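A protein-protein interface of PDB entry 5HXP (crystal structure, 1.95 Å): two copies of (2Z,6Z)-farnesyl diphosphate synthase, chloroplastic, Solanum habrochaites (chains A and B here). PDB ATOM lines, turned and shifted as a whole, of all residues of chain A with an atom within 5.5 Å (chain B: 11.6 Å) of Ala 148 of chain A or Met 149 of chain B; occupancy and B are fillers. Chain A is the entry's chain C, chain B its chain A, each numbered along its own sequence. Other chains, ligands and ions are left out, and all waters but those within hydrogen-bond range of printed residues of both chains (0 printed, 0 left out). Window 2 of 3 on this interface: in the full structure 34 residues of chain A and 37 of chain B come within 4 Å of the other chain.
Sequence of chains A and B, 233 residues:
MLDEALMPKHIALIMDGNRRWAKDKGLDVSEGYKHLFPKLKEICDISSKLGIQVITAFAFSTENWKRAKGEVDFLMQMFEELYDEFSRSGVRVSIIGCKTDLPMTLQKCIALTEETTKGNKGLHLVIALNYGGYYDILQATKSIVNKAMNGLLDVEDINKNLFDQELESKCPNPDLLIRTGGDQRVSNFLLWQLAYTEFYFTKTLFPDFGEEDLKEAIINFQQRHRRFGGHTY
Ala 148 of chain A touches just these residues of chain B: Val 145 (3.6 Å) and Met 149 (3.3 Å).
Of chain A, only Ala 148 (3.3 Å) and Met 149 (3.6 Å) come within 4 Å of Met 149 of chain B.
Val 145 of chain A touches four residues of chain B.
No residue of chain B comes within 4 Å of Asn 146 of chain A.
No residue of chain B comes within 4 Å of Asn 150 of chain A.
No residue of chain B comes within 4 Å of Gly 151 of chain A.
No residue of chain B comes within 4 Å of Leu 152 of chain A.
No residue of chain B comes within 4 Å of Leu 153 of chain A.
Printed residues of chain A within 4 Å of Val 145 of chain B: Val 145, Ala 148 and Val 155.
Printed residues of chain A within 4 Å of Asn 146 of chain B: Val 155.
Of the printed residues of chain A, Val 155 of chain B touches Val 145.
Printed residues of chain B within 4 Å of Val 155 of chain A: Lys 142, Val 145 and Asn 146.
Lys 147 of chain B touches none of the printed residues of chain A.
The nearest printed residue of chain A that does not touch Asn 146 of chain B is Val 145 of chain A (6.7 Å).
Of the 21 printed residues of chain B, 7 touch a printed residue of chain A.
Hydrophobic or aromatic side chains of chain B that line the printed part of chain A: Val 145, Ala 148, Met 149, Val 155 and Ile 158.
Printed residues of chain A that touch a printed residue of chain B: Val 145, Ala 148, Met 149 and Val 155.
Val 145 of chain B touches its own counterpart, Val 145 of chain A.
Val 145 of chain A touches Ala 148 of chain B, and with the chains exchanged Ala 148 of chain A touches Val 145 of chain B.
Ala 148 of chain A touches Met 149 of chain B, and with the chains exchanged Met 149 of chain A touches Ala 148 of chain B.
Val 155 of chain A touches Asn 146 of chain B, but with the chains exchanged Asn 146 of chain A does not touch Val 155 of chain B (4.4 Å).
Positions printed for both chains: 143, 144, 145, 146, 147, 148, 149, 150, 151, 152, 153 and 155.
CG2 of Val 145 of chain A touches CG2 of Val 145 of chain B, at 3.7 Å.
Val 145 of chain A touches Ala 148 of chain B.
Val 155 of chain B touches Val 145 of chain A (CG2 to CG1, 3.4 Å).
Ile 158 of chain B touches Val 145 of chain A (CD1 to CG2, 3.6 Å).
Val 145 of chain B touches Ala 148 of chain A (CG1 to CB, 3.6 Å).
O of Ala 148 of chain A touches CE of Met 149 of chain B, 3.3 Å away.
CE of Met 149 of chain A touches O of Ala 148 of chain B, 3.9 Å away.
Met 149 of chain A touches Met 149 of chain B (CG to CE, 3.6 Å).
Val 145 of chain B touches Val 155 of chain A (CG1 to CG2, 3.5 Å).
Val 155 of chain A touches Asn 146 of chain B (CG2 to OD1, 3.4 Å).
The side-chain amide oxygen of Asn 150 of chain B sits close to the backbone carbonyl oxygen of Asn 146 of chain B.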
ATOM      1  N   SER A 143       2.827  22.117 -13.582  1.00  0.00           N
ATOM      2  CA  SER A 143       1.757  21.204 -13.965  1.00  0.00           C
ATOM      3  C   SER A 143       1.145  21.561 -15.331  1.00  0.00           C
ATOM      4  O   SER A 143       0.934  20.682 -16.171  1.00  0.00           O
ATOM      5  CB  SER A 143       0.683  21.173 -12.871  1.00  0.00           C
ATOM      6  OG  SER A 143      -0.471  20.523 -13.322  1.00  0.00           O
ATOM      7  N   ILE A 144       0.878  22.850 -15.549  1.00  0.00           N
ATOM      8  CA  ILE A 144       0.337  23.334 -16.822  1.00  0.00           C
ATOM      9  C   ILE A 144       1.318  23.082 -17.983  1.00  0.00           C
ATOM     10  O   ILE A 144       0.917  22.602 -19.069  1.00  0.00           O
ATOM     11  CB  ILE A 144      -0.073  24.815 -16.732  1.00  0.00           C
ATOM     12  CG1 ILE A 144      -1.257  24.974 -15.762  1.00  0.00           C
ATOM     13  CG2 ILE A 144      -0.426  25.372 -18.107  1.00  0.00           C
ATOM     14  CD1 ILE A 144      -1.452  26.394 -15.280  1.00  0.00           C
ATOM     15  N   VAL A 145       2.597  23.370 -17.745  1.00  0.00           N
ATOM     16  CA  VAL A 145       3.639  23.091 -18.724  1.00  0.00           C
ATOM     17  C   VAL A 145       3.684  21.579 -19.036  1.00  0.00           C
ATOM     18  O   VAL A 145       3.742  21.191 -20.206  1.00  0.00           O
ATOM     19  CB  VAL A 145       5.029  23.619 -18.273  1.00  0.00           C
ATOM     20  CG1 VAL A 145       6.133  23.098 -19.185  1.00  0.00           C
ATOM     21  CG2 VAL A 145       5.044  25.148 -18.263  1.00  0.00           C
ATOM     22  N   ASN A 146       3.616  20.727 -18.015  1.00  0.00           N
ATOM     23  CA  ASN A 146       3.647  19.287 -18.270  1.00  0.00           C
ATOM     24  C   ASN A 146       2.456  18.858 -19.132  1.00  0.00           C
ATOM     25  O   ASN A 146       2.614  18.085 -20.086  1.00  0.00           O
ATOM     26  CB  ASN A 146       3.699  18.476 -16.972  1.00  0.00           C
ATOM     27  CG  ASN A 146       3.758  16.987 -17.228  1.00  0.00           C
ATOM     28  OD1 ASN A 146       4.818  16.440 -17.548  1.00  0.00           O
ATOM     29  ND2 ASN A 146       2.614  16.315 -17.098  1.00  0.00           N
ATOM     30  N   LYS A 147       1.275  19.372 -18.804  1.00  0.00           N
ATOM     31  CA  LYS A 147       0.062  19.063 -19.565  1.00  0.00           C
ATOM     32  C   LYS A 147       0.123  19.575 -21.009  1.00  0.00           C
ATOM     33  O   LYS A 147      -0.361  18.910 -21.927  1.00  0.00           O
ATOM     34  CB  LYS A 147      -1.169  19.619 -18.859  1.00  0.00           C
ATOM     35  CG  LYS A 147      -1.492  18.885 -17.574  1.00  0.00           C
ATOM     36  CD  LYS A 147      -2.698  19.485 -16.881  1.00  0.00           C
ATOM     37  CE  LYS A 147      -2.902  18.829 -15.528  1.00  0.00           C
ATOM     38  NZ  LYS A 147      -4.150  19.305 -14.886  1.00  0.00           N
ATOM     39  N   ALA A 148       0.721  20.745 -21.216  1.00  0.00           N
ATOM     40  CA  ALA A 148       0.850  21.285 -22.565  1.00  0.00           C
ATOM     41  C   ALA A 148       1.820  20.448 -23.409  1.00  0.00           C
ATOM     42  O   ALA A 148       1.568  20.226 -24.582  1.00  0.00           O
ATOM     43  CB  ALA A 148       1.288  22.746 -22.536  1.00  0.00           C
ATOM     44  N   MET A 149       2.915  19.992 -22.805  1.00  0.00           N
ATOM     45  CA  MET A 149       3.925  19.190 -23.505  1.00  0.00           C
ATOM     46  C   MET A 149       3.496  17.748 -23.803  1.00  0.00           C
ATOM     47  O   MET A 149       4.061  17.100 -24.681  1.00  0.00           O
ATOM     48  CB  MET A 149       5.258  19.221 -22.745  1.00  0.00           C
ATOM     49  CG  MET A 149       6.041  20.506 -23.004  1.00  0.00           C
ATOM     50  SD  MET A 149       7.432  20.717 -21.891  1.00  0.00           S
ATOM     51  CE  MET A 149       8.750  19.948 -22.836  1.00  0.00           C
ATOM     52  N   ASN A 150       2.494  17.260 -23.087  1.00  0.00           N
ATOM     53  CA  ASN A 150       1.907  15.957 -23.348  1.00  0.00           C
ATOM     54  C   ASN A 150       0.605  16.050 -24.158  1.00  0.00           C
ATOM     55  O   ASN A 150      -0.114  15.064 -24.295  1.00  0.00           O
ATOM     56  CB  ASN A 150       1.660  15.238 -22.022  1.00  0.00           C
ATOM     57  CG  ASN A 150       2.936  14.705 -21.407  1.00  0.00           C
ATOM     58  OD1 ASN A 150       3.522  13.755 -21.923  1.00  0.00           O
ATOM     59  ND2 ASN A 150       3.375  15.301 -20.300  1.00  0.00           N
ATOM     60  N   GLY A 151       0.299  17.235 -24.677  1.00  0.00           N
ATOM     61  CA  GLY A 151      -0.870  17.428 -25.534  1.00  0.00           C
ATOM     62  C   GLY A 151      -2.211  17.442 -24.822  1.00  0.00           C
ATOM     63  O   GLY A 151      -3.248  17.205 -25.449  1.00  0.00           O
ATOM     64  N   LEU A 152      -2.211  17.721 -23.520  1.00  0.00           N
ATOM     65  CA  LEU A 152      -3.443  17.676 -22.736  1.00  0.00           C
ATOM     66  C   LEU A 152      -4.110  19.047 -22.647  1.00  0.00           C
ATOM     67  O   LEU A 152      -5.246  19.157 -22.191  1.00  0.00           O
ATOM     68  CB  LEU A 152      -3.172  17.107 -21.343  1.00  0.00           C
ATOM     69  CG  LEU A 152      -2.484  15.730 -21.322  1.00  0.00           C
ATOM     70  CD1 LEU A 152      -2.153  15.287 -19.904  1.00  0.00           C
ATOM     71  CD2 LEU A 152      -3.354  14.696 -22.013  1.00  0.00           C
ATOM     72  N   LEU A 153      -3.419  20.090 -23.094  1.00  0.00           N
ATOM     73  CA  LEU A 153      -4.040  21.398 -23.225  1.00  0.00           C
ATOM     74  C   LEU A 153      -3.236  22.297 -24.146  1.00  0.00           C
ATOM     75  O   LEU A 153      -2.065  22.044 -24.382  1.00  0.00           O
ATOM     76  CB  LEU A 153      -4.228  22.063 -21.850  1.00  0.00           C
ATOM     77  CG  LEU A 153      -2.991  22.427 -21.025  1.00  0.00           C
ATOM     78  CD1 LEU A 153      -2.332  23.703 -21.527  1.00  0.00           C
ATOM     79  CD2 LEU A 153      -3.365  22.575 -19.554  1.00  0.00           C
ATOM     80  N   VAL A 155      -2.095  26.456 -25.102  1.00  0.00           N
ATOM     81  CA  VAL A 155      -1.819  27.758 -24.478  1.00  0.00           C
ATOM     82  C   VAL A 155      -3.069  28.653 -24.425  1.00  0.00           C
ATOM     83  O   VAL A 155      -3.187  29.511 -23.541  1.00  0.00           O
ATOM     84  CB  VAL A 155      -0.670  28.510 -25.205  1.00  0.00           C
ATOM     85  CG1 VAL A 155      -0.428  29.883 -24.588  1.00  0.00           C
ATOM     86  CG2 VAL A 155       0.621  27.704 -25.174  1.00  0.00           C
ATOM     87  N   ALA B 140       2.605  35.551 -17.963  1.00  0.00           N
ATOM     88  CA  ALA B 140       3.913  34.957 -17.709  1.00  0.00           C
ATOM     89  C   ALA B 140       3.867  33.439 -17.912  1.00  0.00           C
ATOM     90  O   ALA B 140       4.755  32.872 -18.545  1.00  0.00           O
ATOM     91  CB  ALA B 140       4.403  35.276 -16.302  1.00  0.00           C
ATOM     92  N   THR B 141       2.844  32.794 -17.346  1.00  0.00           N
ATOM     93  CA  THR B 141       2.660  31.356 -17.485  1.00  0.00           C
ATOM     94  C   THR B 141       2.607  30.939 -18.968  1.00  0.00           C
ATOM     95  O   THR B 141       3.266  29.970 -19.373  1.00  0.00           O
ATOM     96  CB  THR B 141       1.392  30.887 -16.751  1.00  0.00           C
ATOM     97  OG1 THR B 141       1.509  31.184 -15.348  1.00  0.00           O
ATOM     98  CG2 THR B 141       1.194  29.387 -16.941  1.00  0.00           C
ATOM     99  N   LYS B 142       1.837  31.690 -19.753  1.00  0.00           N
ATOM    100  CA  LYS B 142       1.713  31.469 -21.183  1.00  0.00           C
ATOM    101  C   LYS B 142       3.053  31.623 -21.913  1.00  0.00           C
ATOM    102  O   LYS B 142       3.372  30.834 -22.814  1.00  0.00           O
ATOM    103  CB  LYS B 142       0.723  32.460 -21.788  1.00  0.00           C
ATOM    104  CG  LYS B 142      -0.733  32.179 -21.452  1.00  0.00           C
ATOM    105  CD  LYS B 142      -1.596  33.280 -22.059  1.00  0.00           C
ATOM    106  CE  LYS B 142      -3.066  33.086 -21.777  1.00  0.00           C
ATOM    107  NZ  LYS B 142      -3.829  34.264 -22.281  1.00  0.00           N
ATOM    108  N   SER B 143       3.793  32.677 -21.558  1.00  0.00           N
ATOM    109  CA  SER B 143       5.117  32.890 -22.110  1.00  0.00           C
ATOM    110  C   SER B 143       6.021  31.679 -21.790  1.00  0.00           C
ATOM    111  O   SER B 143       6.704  31.169 -22.677  1.00  0.00           O
ATOM    112  CB  SER B 143       5.701  34.196 -21.590  1.00  0.00           C
ATOM    113  OG  SER B 143       7.068  34.314 -21.922  1.00  0.00           O
ATOM    114  N   ILE B 144       5.988  31.200 -20.548  1.00  0.00           N
ATOM    115  CA  ILE B 144       6.775  30.037 -20.137  1.00  0.00           C
ATOM    116  C   ILE B 144       6.359  28.791 -20.933  1.00  0.00           C
ATOM    117  O   ILE B 144       7.224  28.040 -21.428  1.00  0.00           O
ATOM    118  CB  ILE B 144       6.696  29.802 -18.609  1.00  0.00           C
ATOM    119  CG1 ILE B 144       7.420  30.937 -17.875  1.00  0.00           C
ATOM    120  CG2 ILE B 144       7.311  28.470 -18.215  1.00  0.00           C
ATOM    121  CD1 ILE B 144       7.069  31.068 -16.420  1.00  0.00           C
ATOM    122  N   VAL B 145       5.049  28.585 -21.078  1.00  0.00           N
ATOM    123  CA  VAL B 145       4.536  27.432 -21.815  1.00  0.00           C
ATOM    124  C   VAL B 145       4.965  27.491 -23.290  1.00  0.00           C
ATOM    125  O   VAL B 145       5.378  26.469 -23.832  1.00  0.00           O
ATOM    126  CB  VAL B 145       2.990  27.286 -21.690  1.00  0.00           C
ATOM    127  CG1 VAL B 145       2.459  26.169 -22.594  1.00  0.00           C
ATOM    128  CG2 VAL B 145       2.587  27.009 -20.250  1.00  0.00           C
ATOM    129  N   ASN B 146       4.885  28.659 -23.928  1.00  0.00           N
ATOM    130  CA  ASN B 146       5.278  28.785 -25.347  1.00  0.00           C
ATOM    131  C   ASN B 146       6.773  28.469 -25.506  1.00  0.00           C
ATOM    132  O   ASN B 146       7.180  27.787 -26.449  1.00  0.00           O
ATOM    133  CB  ASN B 146       5.002  30.184 -25.925  1.00  0.00           C
ATOM    134  CG  ASN B 146       3.574  30.367 -26.438  1.00  0.00           C
ATOM    135  OD1 ASN B 146       2.913  29.427 -26.908  1.00  0.00           O
ATOM    136  ND2 ASN B 146       3.096  31.606 -26.374  1.00  0.00           N
ATOM    137  N   LYS B 147       7.575  28.954 -24.564  1.00  0.00           N
ATOM    138  CA  LYS B 147       9.000  28.678 -24.565  1.00  0.00           C
ATOM    139  C   LYS B 147       9.282  27.189 -24.393  1.00  0.00           C
ATOM    140  O   LYS B 147      10.118  26.641 -25.101  1.00  0.00           O
ATOM    141  CB  LYS B 147       9.717  29.501 -23.503  1.00  0.00           C
ATOM    142  CG  LYS B 147       9.821  30.964 -23.887  1.00  0.00           C
ATOM    143  CD  LYS B 147      10.509  31.798 -22.823  1.00  0.00           C
ATOM    144  CE  LYS B 147      10.393  33.275 -23.177  1.00  0.00           C
ATOM    145  NZ  LYS B 147      11.161  34.120 -22.231  1.00  0.00           N
ATOM    146  N   ALA B 148       8.583  26.545 -23.465  1.00  0.00           N
ATOM    147  CA  ALA B 148       8.715  25.110 -23.254  1.00  0.00           C
ATOM    148  C   ALA B 148       8.247  24.314 -24.476  1.00  0.00           C
ATOM    149  O   ALA B 148       8.851  23.297 -24.809  1.00  0.00           O
ATOM    150  CB  ALA B 148       7.953  24.672 -22.006  1.00  0.00           C
ATOM    151  N   MET B 149       7.188  24.787 -25.129  1.00  0.00           N
ATOM    152  CA  MET B 149       6.675  24.168 -26.362  1.00  0.00           C
ATOM    153  C   MET B 149       7.673  24.267 -27.516  1.00  0.00           C
ATOM    154  O   MET B 149       7.762  23.359 -28.342  1.00  0.00           O
ATOM    155  CB  MET B 149       5.373  24.834 -26.816  1.00  0.00           C
ATOM    156  CG  MET B 149       4.253  24.851 -25.787  1.00  0.00           C
ATOM    157  SD  MET B 149       3.082  23.509 -25.947  1.00  0.00           S
ATOM    158  CE  MET B 149       4.124  22.121 -25.535  1.00  0.00           C
ATOM    159  N   ASN B 150       8.402  25.379 -27.573  1.00  0.00           N
ATOM    160  CA  ASN B 150       9.419  25.597 -28.589  1.00  0.00           C
ATOM    161  C   ASN B 150      10.794  25.053 -28.191  1.00  0.00           C
ATOM    162  O   ASN B 150      11.773  25.357 -28.854  1.00  0.00           O
ATOM    163  CB  ASN B 150       9.531  27.091 -28.907  1.00  0.00           C
ATOM    164  CG  ASN B 150       8.348  27.609 -29.692  1.00  0.00           C
ATOM    165  OD1 ASN B 150       7.570  28.433 -29.204  1.00  0.00           O
ATOM    166  ND2 ASN B 150       8.198  27.126 -30.917  1.00  0.00           N
ATOM    167  N   GLY B 151      10.861  24.256 -27.127  1.00  0.00           N
ATOM    168  CA  GLY B 151      12.117  23.678 -26.650  1.00  0.00           C
ATOM    169  C   GLY B 151      13.158  24.674 -26.163  1.00  0.00           C
ATOM    170  O   GLY B 151      14.364  24.412 -26.247  1.00  0.00           O
ATOM    171  N   LEU B 152      12.700  25.810 -25.641  1.00  0.00           N
ATOM    172  CA  LEU B 152      13.593  26.878 -25.200  1.00  0.00           C
ATOM    173  C   LEU B 152      13.830  26.849 -23.701  1.00  0.00           C
ATOM    174  O   LEU B 152      14.674  27.582 -23.197  1.00  0.00           O
ATOM    175  CB  LEU B 152      13.048  28.241 -25.631  1.00  0.00           C
ATOM    176  CG  LEU B 152      12.984  28.437 -27.146  1.00  0.00           C
ATOM    177  CD1 LEU B 152      12.050  29.579 -27.528  1.00  0.00           C
ATOM    178  CD2 LEU B 152      14.375  28.661 -27.724  1.00  0.00           C
ATOM    179  N   LEU B 153      13.088  26.007 -22.994  1.00  0.00           N
ATOM    180  CA  LEU B 153      13.348  25.721 -21.585  1.00  0.00           C
ATOM    181  C   LEU B 153      12.668  24.421 -21.173  1.00  0.00           C
ATOM    182  O   LEU B 153      11.831  23.888 -21.902  1.00  0.00           O
ATOM    183  CB  LEU B 153      12.881  26.877 -20.685  1.00  0.00           C
ATOM    184  CG  LEU B 153      11.433  27.360 -20.773  1.00  0.00           C
ATOM    185  CD1 LEU B 153      10.459  26.336 -20.220  1.00  0.00           C
ATOM    186  CD2 LEU B 153      11.275  28.675 -20.022  1.00  0.00           C
ATOM    187  N   ASP B 154      13.022  23.925 -19.996  1.00  0.00           N
ATOM    188  CA  ASP B 154      12.426  22.709 -19.450  1.00  0.00           C
ATOM    189  C   ASP B 154      11.623  23.056 -18.202  1.00  0.00           C
ATOM    190  O   ASP B 154      11.795  24.128 -17.631  1.00  0.00           O
ATOM    191  CB  ASP B 154      13.525  21.701 -19.104  1.00  0.00           C
ATOM    192  CG  ASP B 154      14.638  21.677 -20.141  1.00  0.00           C
ATOM    193  OD1 ASP B 154      14.583  20.815 -21.039  1.00  0.00           O
ATOM    194  OD2 ASP B 154      15.548  22.540 -20.072  1.00  0.00           O
ATOM    195  N   VAL B 155      10.769  22.139 -17.765  1.00  0.00           N
ATOM    196  CA  VAL B 155      10.033  22.317 -16.514  1.00  0.00           C
ATOM    197  C   VAL B 155      11.014  22.572 -15.362  1.00  0.00           C
ATOM    198  O   VAL B 155      10.732  23.379 -14.471  1.00  0.00           O
ATOM    199  CB  VAL B 155       9.144  21.093 -16.193  1.00  0.00           C
ATOM    200  CG1 VAL B 155       8.629  21.146 -14.765  1.00  0.00           C
ATOM    201  CG2 VAL B 155       7.971  21.012 -17.154  1.00  0.00           C
ATOM    202  N   GLU B 156      12.160  21.885 -15.408  1.00  0.00           N
ATOM    203  CA  GLU B 156      13.277  22.068 -14.449  1.00  0.00           C
ATOM    204  C   GLU B 156      13.765  23.509 -14.291  1.00  0.00           C
ATOM    205  O   GLU B 156      14.315  23.862 -13.247  1.00  0.00           O
ATOM    206  CB  GLU B 156      14.500  21.235 -14.885  1.00  0.00           C
ATOM    207  CG  GLU B 156      14.440  19.752 -14.572  1.00  0.00           C
ATOM    208  CD  GLU B 156      13.401  19.002 -15.380  1.00  0.00           C
ATOM    209  OE1 GLU B 156      13.175  19.358 -16.567  1.00  0.00           O
ATOM    210  OE2 GLU B 156      12.808  18.055 -14.816  1.00  0.00           O
ATOM    211  N   ASP B 157      13.617  24.315 -15.336  1.00  0.00           N
ATOM    212  CA  ASP B 157      14.019  25.716 -15.311  1.00  0.00           C
ATOM    213  C   ASP B 157      12.977  26.656 -14.677  1.00  0.00           C
ATOM    214  O   ASP B 157      13.220  27.854 -14.559  1.00  0.00           O
ATOM    215  CB  ASP B 157      14.317  26.196 -16.736  1.00  0.00           C
ATOM    216  CG  ASP B 157      15.518  25.490 -17.368  1.00  0.00           C
ATOM    217  OD1 ASP B 157      16.515  25.229 -16.643  1.00  0.00           O
ATOM    218  OD2 ASP B 157      15.473  25.221 -18.598  1.00  0.00           O
ATOM    219  N   ILE B 158      11.826  26.127 -14.273  1.00  0.00           N
ATOM    220  CA  ILE B 158      10.727  26.977 -13.813  1.00  0.00           C
ATOM    221  C   ILE B 158      10.881  27.246 -12.328  1.00  0.00           C
ATOM    222  O   ILE B 158      10.526  26.434 -11.489  1.00  0.00           O
ATOM    223  CB  ILE B 158       9.361  26.361 -14.125  1.00  0.00           C
ATOM    224  CG1 ILE B 158       9.252  26.131 -15.639  1.00  0.00           C
ATOM    225  CG2 ILE B 158       8.240  27.269 -13.596  1.00  0.00           C
ATOM    226  CD1 ILE B 158       7.964  25.492 -16.101  1.00  0.00           C
ATOM    227  N   LEU B 162      13.006  32.877 -12.778  1.00  0.00           N
ATOM    228  CA  LEU B 162      12.423  32.847 -14.111  1.00  0.00           C
ATOM    229  C   LEU B 162      11.121  33.638 -14.116  1.00  0.00           C
ATOM    230  O   LEU B 162      10.883  34.499 -14.948  1.00  0.00           O
ATOM    231  CB  LEU B 162      12.138  31.412 -14.555  1.00  0.00           C
ATOM    232  CG  LEU B 162      11.492  31.306 -15.942  1.00  0.00           C
ATOM    233  CD1 LEU B 162      12.523  31.595 -17.005  1.00  0.00           C
ATOM    234  CD2 LEU B 162      10.882  29.941 -16.173  1.00  0.00           C
ATOM    235  N   GLU B 166       9.602  37.071 -16.236  1.00  0.00           N
ATOM    236  CA  GLU B 166       8.467  37.041 -17.191  1.00  0.00           C
ATOM    237  C   GLU B 166       7.297  37.966 -16.800  1.00  0.00           C
ATOM    238  O   GLU B 166       6.420  38.239 -17.630  1.00  0.00           O
ATOM    239  CB  GLU B 166       7.915  35.620 -17.344  1.00  0.00           C
ATOM    240  CG  GLU B 166       8.893  34.593 -17.895  1.00  0.00           C
ATOM    241  CD  GLU B 166       9.222  34.780 -19.367  1.00  0.00           C
ATOM    242  OE1 GLU B 166       8.516  35.529 -20.091  1.00  0.00           O
ATOM    243  OE2 GLU B 166      10.211  34.156 -19.804  1.00  0.00           O
